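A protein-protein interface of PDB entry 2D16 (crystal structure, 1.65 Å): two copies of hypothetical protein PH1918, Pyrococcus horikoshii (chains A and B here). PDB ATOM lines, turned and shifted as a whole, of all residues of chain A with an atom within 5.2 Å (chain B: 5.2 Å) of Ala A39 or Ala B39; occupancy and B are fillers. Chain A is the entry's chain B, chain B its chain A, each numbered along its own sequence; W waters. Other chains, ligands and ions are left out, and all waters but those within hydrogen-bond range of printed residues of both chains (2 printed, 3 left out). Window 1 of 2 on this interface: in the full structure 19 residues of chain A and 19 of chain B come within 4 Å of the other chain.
ND2 of Asn A94 is in hydrogen-bond range of O of Thr B38 (2.6 Å).
The backbone carbonyl oxygen (O) of Thr A38 sits at hydrogen-bond distance from the side-chain amide nitrogen (ND2) of Asn B94, 2.6 Å away.
The side-chain amide nitrogen of Asn B94 lies within hydrogen-bond range of the backbone carbonyl oxygen of Ala A39 (3.5 Å).
Of the 10 printed residues of chain B, 5 touch a printed residue of chain A.
Printed residues of chain B that touch a printed residue of chain A: Thr B38, Ala B39, Val B40, Pro B41 and Asn B94.
Of the 10 printed residues of chain A, 5 touch a printed residue of chain B.
Hydrophobic or aromatic side chains of chain A that line the printed part of chain B: Pro A41.
Among the printed residues, no Asp or Glu carboxylate lies within 4 Å of a Lys or Arg side-chain nitrogen of the other chain.
Of chain B, only Ala B39 and Asn B94 come within 4 Å of Ala A39.
Of the printed residues of chain A, Ala B39 touches Ala A39 (3.9 Å) and Asn A94 (3.5 Å).
Of the printed residues of chain B, Thr A38 touches Asn B94 (2.6 Å).
Of the printed residues of chain A, Asn B94 touches Thr A38 (2.6 Å), Ala A39 (3.5 Å), Val A40 (3.8 Å) and Pro A41 (3.1 Å).
Of the printed residues of chain A, Val B40 touches Asn A94.
Printed residues of chain A within 4 Å of Thr B38: Asn A94.
Val B95 touches none of the printed residues of chain A.
Leu B36 touches none of the printed residues of chain A.
The nearest residue of chain A that does not touch Ala B39 is Val A40 (4.02 Å).
Ala A39 touches its own counterpart, Ala B39.
Ala A39 touches Asn B94, and with the chains exchanged Asn A94 touches Ala B39.
Val A40 touches Asn B94, and with the chains exchanged Asn A94 touches Val B40.
Pro A41 touches Asn B94, and with the chains exchanged Asn A94 touches Pro B41.
The backbone carbonyl oxygen of Ala B35 is in hydrogen-bond range of the side-chain hydroxyl of Thr B38, 2.7 Å away.
The backbone carbonyl oxygen (O) of Ala A35 is in hydrogen-bond range of the side-chain hydroxyl (OG1) of Thr A38 (2.6 Å).
Among the printed residues, pairs that only touch across the chains: Ala A39 with Ala B39 (3.9 Å), Val A40 with Asn B94 (3.8 Å), Pro A41 with Asn B94 (3.1 Å), Asn A94 with Ala B39 (3.5 Å), Asn A94 with Val B40 (3.96 Å) and Asn A94 with Pro B41 (3.1 Å).
Water W1 lies within hydrogen-bond range of the backbone carbonyl oxygen (O) of Leu B37 (2.9 Å) and the side-chain amide nitrogen (ND2) of Asn A94 (2.9 Å).
Water W2 lies within hydrogen-bond range of O of Leu A37 (3.0 Å) and ND2 of Asn B94 (3.0 Å).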
ATOM      1  N   ALA A  35      -1.171   1.534  16.803  1.00  0.00           N
ATOM      2  CA  ALA A  35      -1.283   2.859  17.408  1.00  0.00           C
ATOM      3  C   ALA A  35       0.052   3.306  18.003  1.00  0.00           C
ATOM      4  O   ALA A  35       0.450   4.463  17.853  1.00  0.00           O
ATOM      5  CB  ALA A  35      -2.362   2.853  18.485  1.00  0.00           C
ATOM      6  N   LEU A  36       0.741   2.395  18.682  1.00  0.00           N
ATOM      7  CA  LEU A  36       2.030   2.728  19.285  1.00  0.00           C
ATOM      8  C   LEU A  36       3.021   3.230  18.240  1.00  0.00           C
ATOM      9  O   LEU A  36       3.830   4.120  18.516  1.00  0.00           O
ATOM     10  CB  LEU A  36       2.615   1.512  20.007  1.00  0.00           C
ATOM     11  CG  LEU A  36       1.958   1.138  21.335  1.00  0.00           C
ATOM     12  CD1 LEU A  36       2.528  -0.182  21.833  1.00  0.00           C
ATOM     13  CD2 LEU A  36       2.202   2.254  22.359  1.00  0.00           C
ATOM     14  N   LEU A  37       2.957   2.660  17.041  1.00  0.00           N
ATOM     15  CA  LEU A  37       3.848   3.072  15.963  1.00  0.00           C
ATOM     16  C   LEU A  37       3.659   4.542  15.592  1.00  0.00           C
ATOM     17  O   LEU A  37       4.584   5.179  15.088  1.00  0.00           O
ATOM     18  CB  LEU A  37       3.623   2.197  14.726  1.00  0.00           C
ATOM     19  CG  LEU A  37       4.128   0.758  14.832  1.00  0.00           C
ATOM     20  CD1 LEU A  37       3.620  -0.058  13.654  1.00  0.00           C
ATOM     21  CD2 LEU A  37       5.654   0.758  14.880  1.00  0.00           C
ATOM     22  N   THR A  38       2.470   5.086  15.850  1.00  0.00           N
ATOM     23  CA  THR A  38       2.191   6.481  15.521  1.00  0.00           C
ATOM     24  C   THR A  38       2.648   7.464  16.600  1.00  0.00           C
ATOM     25  O   THR A  38       2.702   8.670  16.359  1.00  0.00           O
ATOM     26  CB  THR A  38       0.679   6.731  15.300  1.00  0.00           C
ATOM     27  OG1 THR A  38      -0.010   6.651  16.556  1.00  0.00           O
ATOM     28  CG2 THR A  38       0.099   5.706  14.337  1.00  0.00           C
ATOM     29  N   ALA A  39       2.978   6.948  17.779  1.00  0.00           N
ATOM     30  CA  ALA A  39       3.378   7.803  18.896  1.00  0.00           C
ATOM     31  C   ALA A  39       4.765   8.416  18.788  1.00  0.00           C
ATOM     32  O   ALA A  39       4.944   9.606  19.043  1.00  0.00           O
ATOM     33  CB  ALA A  39       3.261   7.031  20.204  1.00  0.00           C
ATOM     34  N   VAL A  40       5.745   7.601  18.416  1.00  0.00           N
ATOM     35  CA  VAL A  40       7.120   8.064  18.302  1.00  0.00           C
ATOM     36  C   VAL A  40       7.825   7.338  17.163  1.00  0.00           C
ATOM     37  O   VAL A  40       7.834   6.109  17.114  1.00  0.00           O
ATOM     38  CB  VAL A  40       7.918   7.794  19.603  1.00  0.00           C
ATOM     39  CG1 VAL A  40       9.369   8.244  19.430  1.00  0.00           C
ATOM     40  CG2 VAL A  40       7.270   8.520  20.781  1.00  0.00           C
ATOM     41  N   PRO A  41       8.418   8.092  16.227  1.00  0.00           N
ATOM     42  CA  PRO A  41       9.121   7.460  15.106  1.00  0.00           C
ATOM     43  C   PRO A  41      10.282   6.618  15.630  1.00  0.00           C
ATOM     44  O   PRO A  41      11.026   7.057  16.509  1.00  0.00           O
ATOM     45  CB  PRO A  41       9.611   8.654  14.287  1.00  0.00           C
ATOM     46  CG  PRO A  41       8.591   9.721  14.588  1.00  0.00           C
ATOM     47  CD  PRO A  41       8.386   9.555  16.073  1.00  0.00           C
ATOM     48  N   ASN A  94       5.563   9.742  26.208  1.00  0.00           N
ATOM     49  CA  ASN A  94       5.329   9.928  24.778  1.00  0.00           C
ATOM     50  C   ASN A  94       4.219   9.018  24.254  1.00  0.00           C
ATOM     51  O   ASN A  94       3.707   9.243  23.160  1.00  0.00           O
ATOM     52  CB  ASN A  94       6.579   9.607  23.941  1.00  0.00           C
ATOM     53  CG  ASN A  94       7.830  10.303  24.431  1.00  0.00           C
ATOM     54  OD1 ASN A  94       8.883   9.686  24.612  1.00  0.00           O
ATOM     55  ND2 ASN A  94       7.713  11.602  24.671  1.00  0.00           N
ATOM     56  N   VAL A  95       3.849   7.995  25.021  1.00  0.00           N
ATOM     57  CA  VAL A  95       2.853   7.046  24.533  1.00  0.00           C
ATOM     58  C   VAL A  95       1.632   6.745  25.387  1.00  0.00           C
ATOM     59  O   VAL A  95       0.690   6.122  24.898  1.00  0.00           O
ATOM     60  CB  VAL A  95       3.508   5.678  24.218  1.00  0.00           C
ATOM     61  CG1 VAL A  95       4.755   5.875  23.358  1.00  0.00           C
ATOM     62  CG2 VAL A  95       3.848   4.953  25.507  1.00  0.00           C
ATOM     63  N   THR A  98      -1.715   7.768  23.862  1.00  0.00           N
ATOM     64  CA  THR A  98      -2.102   6.945  22.716  1.00  0.00           C
ATOM     65  C   THR A  98      -2.827   5.690  23.212  1.00  0.00           C
ATOM     66  O   THR A  98      -3.843   5.269  22.643  1.00  0.00           O
ATOM     67  CB  THR A  98      -0.858   6.517  21.897  1.00  0.00           C
ATOM     68  OG1 THR A  98      -0.271   7.671  21.283  1.00  0.00           O
ATOM     69  CG2 THR A  98      -1.240   5.505  20.818  1.00  0.00           C
ATOM     70  N   ALA B  35       4.305  21.390  26.271  1.00  0.00           N
ATOM     71  CA  ALA B  35       3.557  20.194  25.903  1.00  0.00           C
ATOM     72  C   ALA B  35       4.197  19.487  24.709  1.00  0.00           C
ATOM     73  O   ALA B  35       4.293  18.260  24.686  1.00  0.00           O
ATOM     74  CB  ALA B  35       2.112  20.562  25.588  1.00  0.00           C
ATOM     75  N   LEU B  36       4.640  20.256  23.719  1.00  0.00           N
ATOM     76  CA  LEU B  36       5.273  19.669  22.536  1.00  0.00           C
ATOM     77  C   LEU B  36       6.521  18.868  22.898  1.00  0.00           C
ATOM     78  O   LEU B  36       6.816  17.843  22.275  1.00  0.00           O
ATOM     79  CB  LEU B  36       5.632  20.759  21.518  1.00  0.00           C
ATOM     80  CG  LEU B  36       4.452  21.332  20.724  1.00  0.00           C
ATOM     81  CD1 LEU B  36       4.889  22.550  19.927  1.00  0.00           C
ATOM     82  CD2 LEU B  36       3.897  20.249  19.802  1.00  0.00           C
ATOM     83  N   LEU B  37       7.257  19.329  23.905  1.00  0.00           N
ATOM     84  CA  LEU B  37       8.456  18.615  24.334  1.00  0.00           C
ATOM     85  C   LEU B  37       8.140  17.204  24.839  1.00  0.00           C
ATOM     86  O   LEU B  37       8.992  16.319  24.785  1.00  0.00           O
ATOM     87  CB  LEU B  37       9.175  19.405  25.432  1.00  0.00           C
ATOM     88  CG  LEU B  37       9.833  20.699  24.953  1.00  0.00           C
ATOM     89  CD1 LEU B  37      10.230  21.563  26.144  1.00  0.00           C
ATOM     90  CD2 LEU B  37      11.044  20.350  24.095  1.00  0.00           C
ATOM     91  N   THR B  38       6.914  16.987  25.316  1.00  0.00           N
ATOM     92  CA  THR B  38       6.531  15.672  25.826  1.00  0.00           C
ATOM     93  C   THR B  38       6.064  14.704  24.736  1.00  0.00           C
ATOM     94  O   THR B  38       5.944  13.502  24.984  1.00  0.00           O
ATOM     95  CB  THR B  38       5.387  15.769  26.869  1.00  0.00           C
ATOM     96  OG1 THR B  38       4.149  16.045  26.201  1.00  0.00           O
ATOM     97  CG2 THR B  38       5.674  16.872  27.879  1.00  0.00           C
ATOM     98  N   ALA B  39       5.811  15.220  23.539  1.00  0.00           N
ATOM     99  CA  ALA B  39       5.319  14.385  22.442  1.00  0.00           C
ATOM    100  C   ALA B  39       6.354  13.452  21.820  1.00  0.00           C
ATOM    101  O   ALA B  39       6.079  12.271  21.616  1.00  0.00           O
ATOM    102  CB  ALA B  39       4.697  15.263  21.366  1.00  0.00           C
ATOM    103  N   VAL B  40       7.537  13.980  21.515  1.00  0.00           N
ATOM    104  CA  VAL B  40       8.600  13.181  20.898  1.00  0.00           C
ATOM    105  C   VAL B  40       9.968  13.614  21.418  1.00  0.00           C
ATOM    106  O   VAL B  40      10.315  14.790  21.356  1.00  0.00           O
ATOM    107  CB  VAL B  40       8.608  13.342  19.349  1.00  0.00           C
ATOM    108  CG1 VAL B  40       9.760  12.540  18.741  1.00  0.00           C
ATOM    109  CG2 VAL B  40       7.276  12.881  18.759  1.00  0.00           C
ATOM    110  N   PRO B  41      10.763  12.667  21.940  1.00  0.00           N
ATOM    111  CA  PRO B  41      12.088  13.038  22.447  1.00  0.00           C
ATOM    112  C   PRO B  41      12.941  13.594  21.314  1.00  0.00           C
ATOM    113  O   PRO B  41      12.968  13.027  20.222  1.00  0.00           O
ATOM    114  CB  PRO B  41      12.640  11.714  22.973  1.00  0.00           C
ATOM    115  CG  PRO B  41      11.399  10.949  23.353  1.00  0.00           C
ATOM    116  CD  PRO B  41      10.481  11.245  22.196  1.00  0.00           C
ATOM    117  N   ASN B  94       2.680  12.498  15.297  1.00  0.00           N
ATOM    118  CA  ASN B  94       3.217  12.271  16.635  1.00  0.00           C
ATOM    119  C   ASN B  94       2.820  13.384  17.604  1.00  0.00           C
ATOM    120  O   ASN B  94       2.936  13.210  18.818  1.00  0.00           O
ATOM    121  CB  ASN B  94       4.754  12.224  16.625  1.00  0.00           C
ATOM    122  CG  ASN B  94       5.321  11.269  15.590  1.00  0.00           C
ATOM    123  OD1 ASN B  94       6.186  11.629  14.786  1.00  0.00           O
ATOM    124  ND2 ASN B  94       4.815  10.041  15.594  1.00  0.00           N
ATOM    125  N   VAL B  95       2.359  14.518  17.082  1.00  0.00           N
ATOM    126  CA  VAL B  95       2.038  15.654  17.952  1.00  0.00           C
ATOM    127  C   VAL B  95       0.652  16.289  17.891  1.00  0.00           C
ATOM    128  O   VAL B  95       0.306  17.082  18.768  1.00  0.00           O
ATOM    129  CB  VAL B  95       3.050  16.806  17.737  1.00  0.00           C
ATOM    130  CG1 VAL B  95       4.479  16.266  17.775  1.00  0.00           C
ATOM    131  CG2 VAL B  95       2.773  17.506  16.424  1.00  0.00           C
ATOM    132  N   THR B  98      -1.472  15.952  21.018  1.00  0.00           N
ATOM    133  CA  THR B  98      -0.958  16.749  22.131  1.00  0.00           C
ATOM    134  C   THR B  98      -1.480  18.184  22.012  1.00  0.00           C
ATOM    135  O   THR B  98      -1.843  18.817  23.010  1.00  0.00           O
ATOM    136  CB  THR B  98       0.591  16.760  22.132  1.00  0.00           C
ATOM    137  OG1 THR B  98       1.071  15.448  22.449  1.00  0.00           O
ATOM    138  CG2 THR B  98       1.131  17.755  23.161  1.00  0.00           C
HETATM  139  O   HOH W   1       9.694  13.588  25.534  1.00  0.00           O
HETATM  140  O   HOH W   2       5.393   7.710  13.776  1.00  0.00           O
